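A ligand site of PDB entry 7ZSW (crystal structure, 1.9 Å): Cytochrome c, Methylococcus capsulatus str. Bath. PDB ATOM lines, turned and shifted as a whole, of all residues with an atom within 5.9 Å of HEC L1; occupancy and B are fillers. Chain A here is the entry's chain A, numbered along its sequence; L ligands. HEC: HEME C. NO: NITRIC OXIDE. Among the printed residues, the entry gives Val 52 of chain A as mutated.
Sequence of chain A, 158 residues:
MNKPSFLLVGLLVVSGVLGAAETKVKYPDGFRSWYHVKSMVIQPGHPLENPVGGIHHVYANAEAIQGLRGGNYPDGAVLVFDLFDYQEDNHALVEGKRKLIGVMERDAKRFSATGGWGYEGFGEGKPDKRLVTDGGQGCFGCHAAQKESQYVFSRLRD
Met 40 touches HEC L1 (CE to O1D, 3.6 Å).
CD2 of Leu 48 touches CBC of HEC L1 (3.9 Å).
Val 58 touches HEC L1 (CG1 to CAA, 3.7 Å).
Leu 79 touches HEC L1 (O to CMA, 3.4 Å).
Phe 81 touches HEC L1 (CD2 to C1A, 3.6 Å).
Gly 102 touches HEC L1.
O of Val 103 touches CMB of HEC L1 (3.7 Å).
Met 104 touches HEC L1.
Tyr 119 touches HEC L1.
O of Glu 120 touches CMB of HEC L1 (3.2 Å).
Val 132 touches HEC L1.
Gly 138 touches HEC L1.
Val 152 touches HEC L1 (CA to O2A, 3.4 Å).
Hydrophobic or aromatic side chains within 4 Å of HEC L1: Met 40, Leu 48, His 56, Val 58, Phe 81, Met 104, Tyr 119, Val 132, His 143, Val 152 and Phe 153.
Of the 27 residues printed, 20 come within 4 Å of HEC L1.
The nearest printed residue that does not touch HEC L1 is Val 80 (4.1 Å).
N of NO L2 binds FE of HEC L1.
OE2 of Glu 120 is in hydrogen-bond range of N of Val 132 (3.1 Å).
The backbone NH (N) of His 56 lies within hydrogen-bond range of the backbone carbonyl oxygen (O) of Met 40, at 2.9 Å.
N of Gly 102 sits at hydrogen-bond distance from O of Phe 81.
The backbone NH (N) of Val 58 sits at hydrogen-bond distance from the backbone carbonyl oxygen (O) of Lys 38 (2.8 Å).
The backbone carbonyl oxygen of Glu 120 is in hydrogen-bond range of the backbone NH of Val 103 (2.8 Å).
N of Met 104 lies within hydrogen-bond range of O of Leu 79 (2.9 Å).
A ring nitrogen (ND1) of His 143 lies close to the side-chain sulfur of Met 104 (3.7 Å).
A ring nitrogen (ND1) of His 143 is in hydrogen-bond range of the backbone carbonyl oxygen (O) of Tyr 151 (2.9 Å).
OG of Ser 154 lies within hydrogen-bond range of O1A of HEC L1 (2.5 Å).
SG of Cys 142 is covalently linked to CAC of HEC L1.
An oxygen (O1D) of HEC L1 sits at hydrogen-bond distance from a ring nitrogen (NE2) of His 56 (2.4 Å).
A ring nitrogen (NE2) of His 143 binds an iron atom (FE) of HEC L1 (2.5 Å).
The backbone NH of Phe 153 lies within hydrogen-bond range of an oxygen (O2A) of HEC L1, at 3.0 Å.
An oxygen (O1A) of HEC L1 lies within hydrogen-bond range of the backbone NH (N) of Ser 154.
The side-chain sulfur (SG) of Cys 139 is bonded to a carbon (CAB) of HEC L1, at 1.7 Å.
The side-chain amino group (NZ) of Lys 38 is in salt-bridge range of an oxygen (O2D) of HEC L1 (2.7 Å).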
ATOM      1  N   LYS A  38     -11.211   3.933  27.648  1.00  0.00           N
ATOM      2  CA  LYS A  38     -11.207   3.321  26.301  1.00  0.00           C
ATOM      3  C   LYS A  38     -10.460   1.994  26.319  1.00  0.00           C
ATOM      4  O   LYS A  38      -9.768   1.701  27.308  1.00  0.00           O
ATOM      5  CB  LYS A  38     -10.541   4.247  25.284  1.00  0.00           C
ATOM      6  CG  LYS A  38      -9.046   4.430  25.481  1.00  0.00           C
ATOM      7  CD  LYS A  38      -8.368   5.147  24.358  1.00  0.00           C
ATOM      8  CE  LYS A  38      -8.482   4.380  23.048  1.00  0.00           C
ATOM      9  NZ  LYS A  38      -7.644   4.989  21.993  1.00  0.00           N
ATOM     10  N   SER A  39     -10.570   1.253  25.231  1.00  0.00           N
ATOM     11  CA  SER A  39      -9.833  -0.010  24.987  1.00  0.00           C
ATOM     12  C   SER A  39      -9.335  -0.022  23.561  1.00  0.00           C
ATOM     13  O   SER A  39      -9.851   0.747  22.726  1.00  0.00           O
ATOM     14  CB  SER A  39     -10.678  -1.190  25.268  1.00  0.00           C
ATOM     15  OG  SER A  39     -11.146  -1.106  26.590  1.00  0.00           O
ATOM     16  N   MET A  40      -8.392  -0.922  23.312  1.00  0.00           N
ATOM     17  CA  MET A  40      -7.803  -1.187  21.980  1.00  0.00           C
ATOM     18  C   MET A  40      -7.161  -2.595  22.019  1.00  0.00           C
ATOM     19  O   MET A  40      -6.732  -3.044  23.127  1.00  0.00           O
ATOM     20  CB  MET A  40      -6.764  -0.121  21.641  1.00  0.00           C
ATOM     21  CG  MET A  40      -6.207  -0.243  20.219  1.00  0.00           C
ATOM     22  SD  MET A  40      -4.826   0.903  19.928  1.00  0.00           S
ATOM     23  CE  MET A  40      -5.712   2.461  20.010  1.00  0.00           C
ATOM     24  N   LEU A  48       3.692  -2.196  17.531  1.00  0.00           N
ATOM     25  CA  LEU A  48       3.804  -2.139  19.022  1.00  0.00           C
ATOM     26  C   LEU A  48       3.530  -3.517  19.672  1.00  0.00           C
ATOM     27  O   LEU A  48       3.451  -3.564  20.935  1.00  0.00           O
ATOM     28  CB  LEU A  48       2.833  -1.065  19.529  1.00  0.00           C
ATOM     29  CG  LEU A  48       3.063   0.377  19.031  1.00  0.00           C
ATOM     30  CD1 LEU A  48       2.117   1.381  19.702  1.00  0.00           C
ATOM     31  CD2 LEU A  48       4.505   0.807  19.251  1.00  0.00           C
ATOM     32  N   VAL A  52       3.511  -4.072  23.932  1.00  0.00           N
ATOM     33  CA  VAL A  52       2.104  -3.765  24.351  1.00  0.00           C
ATOM     34  C   VAL A  52       1.098  -4.569  23.521  1.00  0.00           C
ATOM     35  O   VAL A  52      -0.097  -4.196  23.506  1.00  0.00           O
ATOM     36  CB  VAL A  52       1.806  -2.253  24.360  1.00  0.00           C
ATOM     37  CG1 VAL A  52       2.634  -1.595  25.459  1.00  0.00           C
ATOM     38  CG2 VAL A  52       2.032  -1.596  23.010  1.00  0.00           C
ATOM     39  N   HIS A  56      -5.770  -3.907  25.743  1.00  0.00           N
ATOM     40  CA  HIS A  56      -5.529  -2.931  26.834  1.00  0.00           C
ATOM     41  C   HIS A  56      -6.782  -2.088  27.092  1.00  0.00           C
ATOM     42  O   HIS A  56      -7.589  -1.838  26.158  1.00  0.00           O
ATOM     43  CB  HIS A  56      -4.263  -2.123  26.607  1.00  0.00           C
ATOM     44  CG  HIS A  56      -4.340  -1.051  25.583  1.00  0.00           C
ATOM     45  ND1 HIS A  56      -3.703  -1.171  24.374  1.00  0.00           N
ATOM     46  CD2 HIS A  56      -4.860   0.189  25.632  1.00  0.00           C
ATOM     47  CE1 HIS A  56      -3.884  -0.055  23.689  1.00  0.00           C
ATOM     48  NE2 HIS A  56      -4.590   0.792  24.443  1.00  0.00           N
ATOM     49  N   VAL A  58      -7.795   1.494  29.294  1.00  0.00           N
ATOM     50  CA  VAL A  58      -7.289   2.702  29.970  1.00  0.00           C
ATOM     51  C   VAL A  58      -8.271   3.093  31.072  1.00  0.00           C
ATOM     52  O   VAL A  58      -9.500   3.099  30.808  1.00  0.00           O
ATOM     53  CB  VAL A  58      -7.052   3.831  28.959  1.00  0.00           C
ATOM     54  CG1 VAL A  58      -6.467   5.056  29.654  1.00  0.00           C
ATOM     55  CG2 VAL A  58      -6.140   3.381  27.818  1.00  0.00           C
ATOM     56  N   LEU A  79      -3.507   7.922  35.325  1.00  0.00           N
ATOM     57  CA  LEU A  79      -3.971   7.130  34.167  1.00  0.00           C
ATOM     58  C   LEU A  79      -3.314   5.754  34.268  1.00  0.00           C
ATOM     59  O   LEU A  79      -2.106   5.701  34.620  1.00  0.00           O
ATOM     60  CB  LEU A  79      -3.543   7.869  32.898  1.00  0.00           C
ATOM     61  CG  LEU A  79      -4.321   9.159  32.664  1.00  0.00           C
ATOM     62  CD1 LEU A  79      -3.589  10.066  31.699  1.00  0.00           C
ATOM     63  CD2 LEU A  79      -5.721   8.839  32.151  1.00  0.00           C
ATOM     64  N   VAL A  80      -4.081   4.702  34.010  1.00  0.00           N
ATOM     65  CA  VAL A  80      -3.560   3.312  34.019  1.00  0.00           C
ATOM     66  C   VAL A  80      -3.815   2.665  32.651  1.00  0.00           C
ATOM     67  O   VAL A  80      -4.963   2.723  32.166  1.00  0.00           O
ATOM     68  CB  VAL A  80      -4.165   2.469  35.149  1.00  0.00           C
ATOM     69  CG1 VAL A  80      -3.620   1.036  35.087  1.00  0.00           C
ATOM     70  CG2 VAL A  80      -3.908   3.103  36.499  1.00  0.00           C
ATOM     71  N   PHE A  81      -2.774   2.062  32.083  1.00  0.00           N
ATOM     72  CA  PHE A  81      -2.792   1.206  30.871  1.00  0.00           C
ATOM     73  C   PHE A  81      -2.773  -0.251  31.346  1.00  0.00           C
ATOM     74  O   PHE A  81      -1.707  -0.673  31.835  1.00  0.00           O
ATOM     75  CB  PHE A  81      -1.573   1.562  30.017  1.00  0.00           C
ATOM     76  CG  PHE A  81      -1.441   0.838  28.695  1.00  0.00           C
ATOM     77  CD1 PHE A  81      -0.915  -0.447  28.617  1.00  0.00           C
ATOM     78  CD2 PHE A  81      -1.721   1.497  27.500  1.00  0.00           C
ATOM     79  CE1 PHE A  81      -0.721  -1.055  27.380  1.00  0.00           C
ATOM     80  CE2 PHE A  81      -1.515   0.893  26.256  1.00  0.00           C
ATOM     81  CZ  PHE A  81      -1.022  -0.399  26.206  1.00  0.00           C
ATOM     82  N   GLY A 102       0.772  -0.053  32.821  1.00  0.00           N
ATOM     83  CA  GLY A 102       1.506   1.211  32.780  1.00  0.00           C
ATOM     84  C   GLY A 102       0.750   2.249  33.606  1.00  0.00           C
ATOM     85  O   GLY A 102      -0.502   2.179  33.645  1.00  0.00           O
ATOM     86  N   VAL A 103       1.475   3.162  34.251  1.00  0.00           N
ATOM     87  CA  VAL A 103       0.882   4.152  35.186  1.00  0.00           C
ATOM     88  C   VAL A 103       1.530   5.501  34.906  1.00  0.00           C
ATOM     89  O   VAL A 103       2.789   5.565  34.784  1.00  0.00           O
ATOM     90  CB  VAL A 103       1.064   3.728  36.651  1.00  0.00           C
ATOM     91  CG1 VAL A 103       0.363   4.699  37.604  1.00  0.00           C
ATOM     92  CG2 VAL A 103       0.596   2.307  36.870  1.00  0.00           C
ATOM     93  N   MET A 104       0.681   6.520  34.732  1.00  0.00           N
ATOM     94  CA  MET A 104       1.119   7.931  34.635  1.00  0.00           C
ATOM     95  C   MET A 104       0.516   8.662  35.826  1.00  0.00           C
ATOM     96  O   MET A 104      -0.679   8.567  36.019  1.00  0.00           O
ATOM     97  CB  MET A 104       0.639   8.565  33.332  1.00  0.00           C
ATOM     98  CG  MET A 104       1.429   8.116  32.135  1.00  0.00           C
ATOM     99  SD  MET A 104       0.614   8.616  30.582  1.00  0.00           S
ATOM    100  CE  MET A 104       0.850  10.396  30.604  1.00  0.00           C
ATOM    101  N   TYR A 119       6.263   8.138  35.126  1.00  0.00           N
ATOM    102  CA  TYR A 119       5.980   6.907  34.359  1.00  0.00           C
ATOM    103  C   TYR A 119       6.536   5.683  35.111  1.00  0.00           C
ATOM    104  O   TYR A 119       7.725   5.634  35.398  1.00  0.00           O
ATOM    105  CB  TYR A 119       6.554   7.039  32.953  1.00  0.00           C
ATOM    106  CG  TYR A 119       5.951   8.134  32.105  1.00  0.00           C
ATOM    107  CD1 TYR A 119       6.436   9.438  32.145  1.00  0.00           C
ATOM    108  CD2 TYR A 119       4.939   7.853  31.208  1.00  0.00           C
ATOM    109  CE1 TYR A 119       5.897  10.437  31.364  1.00  0.00           C
ATOM    110  CE2 TYR A 119       4.402   8.843  30.395  1.00  0.00           C
ATOM    111  CZ  TYR A 119       4.861  10.144  30.494  1.00  0.00           C
ATOM    112  OH  TYR A 119       4.305  11.111  29.711  1.00  0.00           O
ATOM    113  N   GLU A 120       5.695   4.673  35.309  1.00  0.00           N
ATOM    114  CA  GLU A 120       6.054   3.370  35.929  1.00  0.00           C
ATOM    115  C   GLU A 120       5.239   2.253  35.298  1.00  0.00           C
ATOM    116  O   GLU A 120       4.119   2.514  34.837  1.00  0.00           O
ATOM    117  CB  GLU A 120       5.827   3.442  37.443  1.00  0.00           C
ATOM    118  CG  GLU A 120       6.166   2.173  38.184  1.00  0.00           C
ATOM    119  CD  GLU A 120       7.654   1.898  38.164  1.00  0.00           C
ATOM    120  OE1 GLU A 120       8.357   2.307  39.125  1.00  0.00           O
ATOM    121  OE2 GLU A 120       8.102   1.313  37.167  1.00  0.00           O
ATOM    122  N   GLY A 121       5.828   1.055  35.261  1.00  0.00           N
ATOM    123  CA  GLY A 121       5.200  -0.220  34.876  1.00  0.00           C
ATOM    124  C   GLY A 121       5.239  -1.187  36.042  1.00  0.00           C
ATOM    125  O   GLY A 121       6.197  -1.141  36.847  1.00  0.00           O
ATOM    126  N   VAL A 132      10.380   0.166  35.456  1.00  0.00           N
ATOM    127  CA  VAL A 132      11.089   1.301  34.817  1.00  0.00           C
ATOM    128  C   VAL A 132      12.425   1.502  35.516  1.00  0.00           C
ATOM    129  O   VAL A 132      12.438   1.578  36.755  1.00  0.00           O
ATOM    130  CB  VAL A 132      10.216   2.576  34.815  1.00  0.00           C
ATOM    131  CG1 VAL A 132      11.046   3.814  34.537  1.00  0.00           C
ATOM    132  CG2 VAL A 132       9.051   2.472  33.825  1.00  0.00           C
ATOM    133  N   GLY A 136      11.882   6.940  33.572  1.00  0.00           N
ATOM    134  CA  GLY A 136      10.711   7.062  32.678  1.00  0.00           C
ATOM    135  C   GLY A 136      11.009   7.855  31.412  1.00  0.00           C
ATOM    136  O   GLY A 136      10.036   8.199  30.700  1.00  0.00           O
ATOM    137  N   GLY A 138      12.378   6.793  28.580  1.00  0.00           N
ATOM    138  CA  GLY A 138      11.865   5.982  27.462  1.00  0.00           C
ATOM    139  C   GLY A 138      10.366   6.192  27.270  1.00  0.00           C
ATOM    140  O   GLY A 138       9.915   6.404  26.129  1.00  0.00           O
ATOM    141  N   CYS A 139       9.590   6.124  28.351  1.00  0.00           N
ATOM    142  CA  CYS A 139       8.117   6.292  28.309  1.00  0.00           C
ATOM    143  C   CYS A 139       7.826   7.674  27.719  1.00  0.00           C
ATOM    144  O   CYS A 139       7.063   7.787  26.714  1.00  0.00           O
ATOM    145  CB  CYS A 139       7.502   6.196  29.704  1.00  0.00           C
ATOM    146  SG  CYS A 139       7.930   4.670  30.530  1.00  0.00           S
ATOM    147  N   PHE A 140       8.416   8.687  28.336  1.00  0.00           N
ATOM    148  CA  PHE A 140       8.287  10.125  28.018  1.00  0.00           C
ATOM    149  C   PHE A 140       8.628  10.355  26.541  1.00  0.00           C
ATOM    150  O   PHE A 140       7.940  11.165  25.919  1.00  0.00           O
ATOM    151  CB  PHE A 140       9.193  10.921  28.951  1.00  0.00           C
ATOM    152  CG  PHE A 140       9.142  12.410  28.743  1.00  0.00           C
ATOM    153  CD1 PHE A 140       7.926  13.057  28.656  1.00  0.00           C
ATOM    154  CD2 PHE A 140      10.310  13.153  28.668  1.00  0.00           C
ATOM    155  CE1 PHE A 140       7.872  14.435  28.489  1.00  0.00           C
ATOM    156  CE2 PHE A 140      10.248  14.523  28.485  1.00  0.00           C
ATOM    157  CZ  PHE A 140       9.033  15.166  28.411  1.00  0.00           C
ATOM    158  N   CYS A 142       8.120   8.522  23.821  1.00  0.00           N
ATOM    159  CA  CYS A 142       6.937   8.249  22.966  1.00  0.00           C
ATOM    160  C   CYS A 142       5.829   9.266  23.296  1.00  0.00           C
ATOM    161  O   CYS A 142       5.258   9.893  22.361  1.00  0.00           O
ATOM    162  CB  CYS A 142       6.504   6.809  23.180  1.00  0.00           C
ATOM    163  SG  CYS A 142       5.563   6.139  21.850  1.00  0.00           S
ATOM    164  N   HIS A 143       5.535   9.482  24.581  1.00  0.00           N
ATOM    165  CA  HIS A 143       4.412  10.333  25.053  1.00  0.00           C
ATOM    166  C   HIS A 143       4.636  11.804  24.638  1.00  0.00           C
ATOM    167  O   HIS A 143       3.637  12.557  24.579  1.00  0.00           O
ATOM    168  CB  HIS A 143       4.142  10.124  26.551  1.00  0.00           C
ATOM    169  CG  HIS A 143       3.354   8.876  26.840  1.00  0.00           C
ATOM    170  ND1 HIS A 143       2.002   8.918  27.173  1.00  0.00           N
ATOM    171  CD2 HIS A 143       3.696   7.574  26.797  1.00  0.00           C
ATOM    172  CE1 HIS A 143       1.567   7.667  27.346  1.00  0.00           C
ATOM    173  NE2 HIS A 143       2.587   6.809  27.094  1.00  0.00           N
ATOM    174  N   TYR A 151       0.546  15.210  26.990  1.00  0.00           N
ATOM    175  CA  TYR A 151       1.311  13.923  26.923  1.00  0.00           C
ATOM    176  C   TYR A 151       0.411  12.687  27.040  1.00  0.00           C
ATOM    177  O   TYR A 151       0.968  11.586  27.275  1.00  0.00           O
ATOM    178  CB  TYR A 151       2.376  13.884  28.019  1.00  0.00           C
ATOM    179  CG  TYR A 151       3.358  14.998  27.880  1.00  0.00           C
ATOM    180  CD1 TYR A 151       4.258  14.987  26.832  1.00  0.00           C
ATOM    181  CD2 TYR A 151       3.357  16.082  28.746  1.00  0.00           C
ATOM    182  CE1 TYR A 151       5.179  16.010  26.666  1.00  0.00           C
ATOM    183  CE2 TYR A 151       4.272  17.113  28.590  1.00  0.00           C
ATOM    184  CZ  TYR A 151       5.171  17.077  27.543  1.00  0.00           C
ATOM    185  OH  TYR A 151       6.100  18.042  27.331  1.00  0.00           O
ATOM    186  N   VAL A 152      -0.903  12.859  26.850  1.00  0.00           N
ATOM    187  CA  VAL A 152      -1.910  11.758  26.935  1.00  0.00           C
ATOM    188  C   VAL A 152      -2.424  11.441  25.527  1.00  0.00           C
ATOM    189  O   VAL A 152      -2.879  12.368  24.863  1.00  0.00           O
ATOM    190  CB  VAL A 152      -3.041  12.146  27.898  1.00  0.00           C
ATOM    191  CG1 VAL A 152      -4.106  11.056  27.942  1.00  0.00           C
ATOM    192  CG2 VAL A 152      -2.503  12.475  29.279  1.00  0.00           C
ATOM    193  N   PHE A 153      -2.289  10.199  25.069  1.00  0.00           N
ATOM    194  CA  PHE A 153      -2.808   9.702  23.771  1.00  0.00           C
ATOM    195  C   PHE A 153      -4.329   9.546  23.817  1.00  0.00           C
ATOM    196  O   PHE A 153      -4.987   9.953  22.891  1.00  0.00           O
ATOM    197  CB  PHE A 153      -2.195   8.346  23.398  1.00  0.00           C
ATOM    198  CG  PHE A 153      -0.736   8.373  23.026  1.00  0.00           C
ATOM    199  CD1 PHE A 153       0.236   8.108  23.983  1.00  0.00           C
ATOM    200  CD2 PHE A 153      -0.325   8.662  21.728  1.00  0.00           C
ATOM    201  CE1 PHE A 153       1.590   8.115  23.650  1.00  0.00           C
ATOM    202  CE2 PHE A 153       1.023   8.681  21.392  1.00  0.00           C
ATOM    203  CZ  PHE A 153       1.986   8.397  22.350  1.00  0.00           C
ATOM    204  N   SER A 154      -4.848   8.920  24.870  1.00  0.00           N
ATOM    205  CA  SER A 154      -6.254   8.490  25.011  1.00  0.00           C
ATOM    206  C   SER A 154      -7.176   9.709  24.949  1.00  0.00           C
ATOM    207  O   SER A 154      -6.836  10.741  25.575  1.00  0.00           O
ATOM    208  CB  SER A 154      -6.470   7.697  26.291  1.00  0.00           C
ATOM    209  OG  SER A 154      -5.687   6.512  26.299  1.00  0.00           O
HETATM  210 FE   HEC L   1       2.289   4.311  26.763  1.00  0.00          FE
HETATM  211  CHA HEC L   1      -1.099   4.897  26.456  1.00  0.00           C
HETATM  212  CHB HEC L   1       2.053   4.463  30.204  1.00  0.00           C
HETATM  213  CHC HEC L   1       5.650   3.696  26.988  1.00  0.00           C
HETATM  214  CHD HEC L   1       2.562   4.549  23.312  1.00  0.00           C
HETATM  215  NA  HEC L   1       0.746   4.625  28.137  1.00  0.00           N
HETATM  216  C1A HEC L   1      -0.553   4.866  27.826  1.00  0.00           C
HETATM  217  C2A HEC L   1      -1.432   5.077  29.006  1.00  0.00           C
HETATM  218  C3A HEC L   1      -0.486   4.999  30.122  1.00  0.00           C
HETATM  219  C4A HEC L   1       0.807   4.699  29.463  1.00  0.00           C
HETATM  220  CMA HEC L   1      -0.789   5.126  31.557  1.00  0.00           C
HETATM  221  CAA HEC L   1      -2.853   5.452  28.988  1.00  0.00           C
HETATM  222  CBA HEC L   1      -2.778   7.009  28.991  1.00  0.00           C
HETATM  223  CGA HEC L   1      -2.575   7.659  27.595  1.00  0.00           C
HETATM  224  O1A HEC L   1      -3.395   7.357  26.690  1.00  0.00           O
HETATM  225  O2A HEC L   1      -1.571   8.404  27.338  1.00  0.00           O
HETATM  226  NB  HEC L   1       3.649   4.123  28.328  1.00  0.00           N
HETATM  227  C1B HEC L   1       3.372   4.167  29.627  1.00  0.00           C
HETATM  228  C2B HEC L   1       4.540   3.910  30.503  1.00  0.00           C
HETATM  229  C3B HEC L   1       5.611   3.696  29.541  1.00  0.00           C
HETATM  230  C4B HEC L   1       4.932   3.820  28.251  1.00  0.00           C
HETATM  231  CMB HEC L   1       4.495   3.908  31.978  1.00  0.00           C
HETATM  232  CAB HEC L   1       7.071   3.358  29.820  1.00  0.00           C
HETATM  233  CBB HEC L   1       7.251   2.002  30.478  1.00  0.00           C
HETATM  234  NC  HEC L   1       3.833   4.156  25.385  1.00  0.00           N
HETATM  235  C1C HEC L   1       5.122   3.932  25.656  1.00  0.00           C
HETATM  236  C2C HEC L   1       6.037   3.915  24.511  1.00  0.00           C
HETATM  237  C3C HEC L   1       5.090   4.137  23.424  1.00  0.00           C
HETATM  238  C4C HEC L   1       3.782   4.322  24.070  1.00  0.00           C
HETATM  239  CMC HEC L   1       7.498   3.682  24.542  1.00  0.00           C
HETATM  240  CAC HEC L   1       5.398   4.361  21.974  1.00  0.00           C
HETATM  241  CBC HEC L   1       6.431   3.508  21.303  1.00  0.00           C
HETATM  242  ND  HEC L   1       0.958   4.636  25.158  1.00  0.00           N
HETATM  243  C1D HEC L   1       1.220   4.678  23.847  1.00  0.00           C
HETATM  244  C2D HEC L   1       0.029   4.830  22.948  1.00  0.00           C
HETATM  245  C3D HEC L   1      -1.072   4.918  23.910  1.00  0.00           C
HETATM  246  C4D HEC L   1      -0.373   4.807  25.210  1.00  0.00           C
HETATM  247  CMD HEC L   1      -0.005   4.909  21.445  1.00  0.00           C
HETATM  248  CAD HEC L   1      -2.511   5.096  23.627  1.00  0.00           C
HETATM  249  CBD HEC L   1      -3.158   3.693  23.662  1.00  0.00           C
HETATM  250  CGD HEC L   1      -4.631   3.786  23.302  1.00  0.00           C
HETATM  251  O1D HEC L   1      -5.437   2.882  23.591  1.00  0.00           O
HETATM  252  O2D HEC L   1      -5.026   4.842  22.742  1.00  0.00           O
HETATM  253  N    NO L   2       1.973   2.456  26.549  1.00  0.00           N
HETATM  254  O    NO L   2       1.734   1.941  27.661  1.00  0.00           O
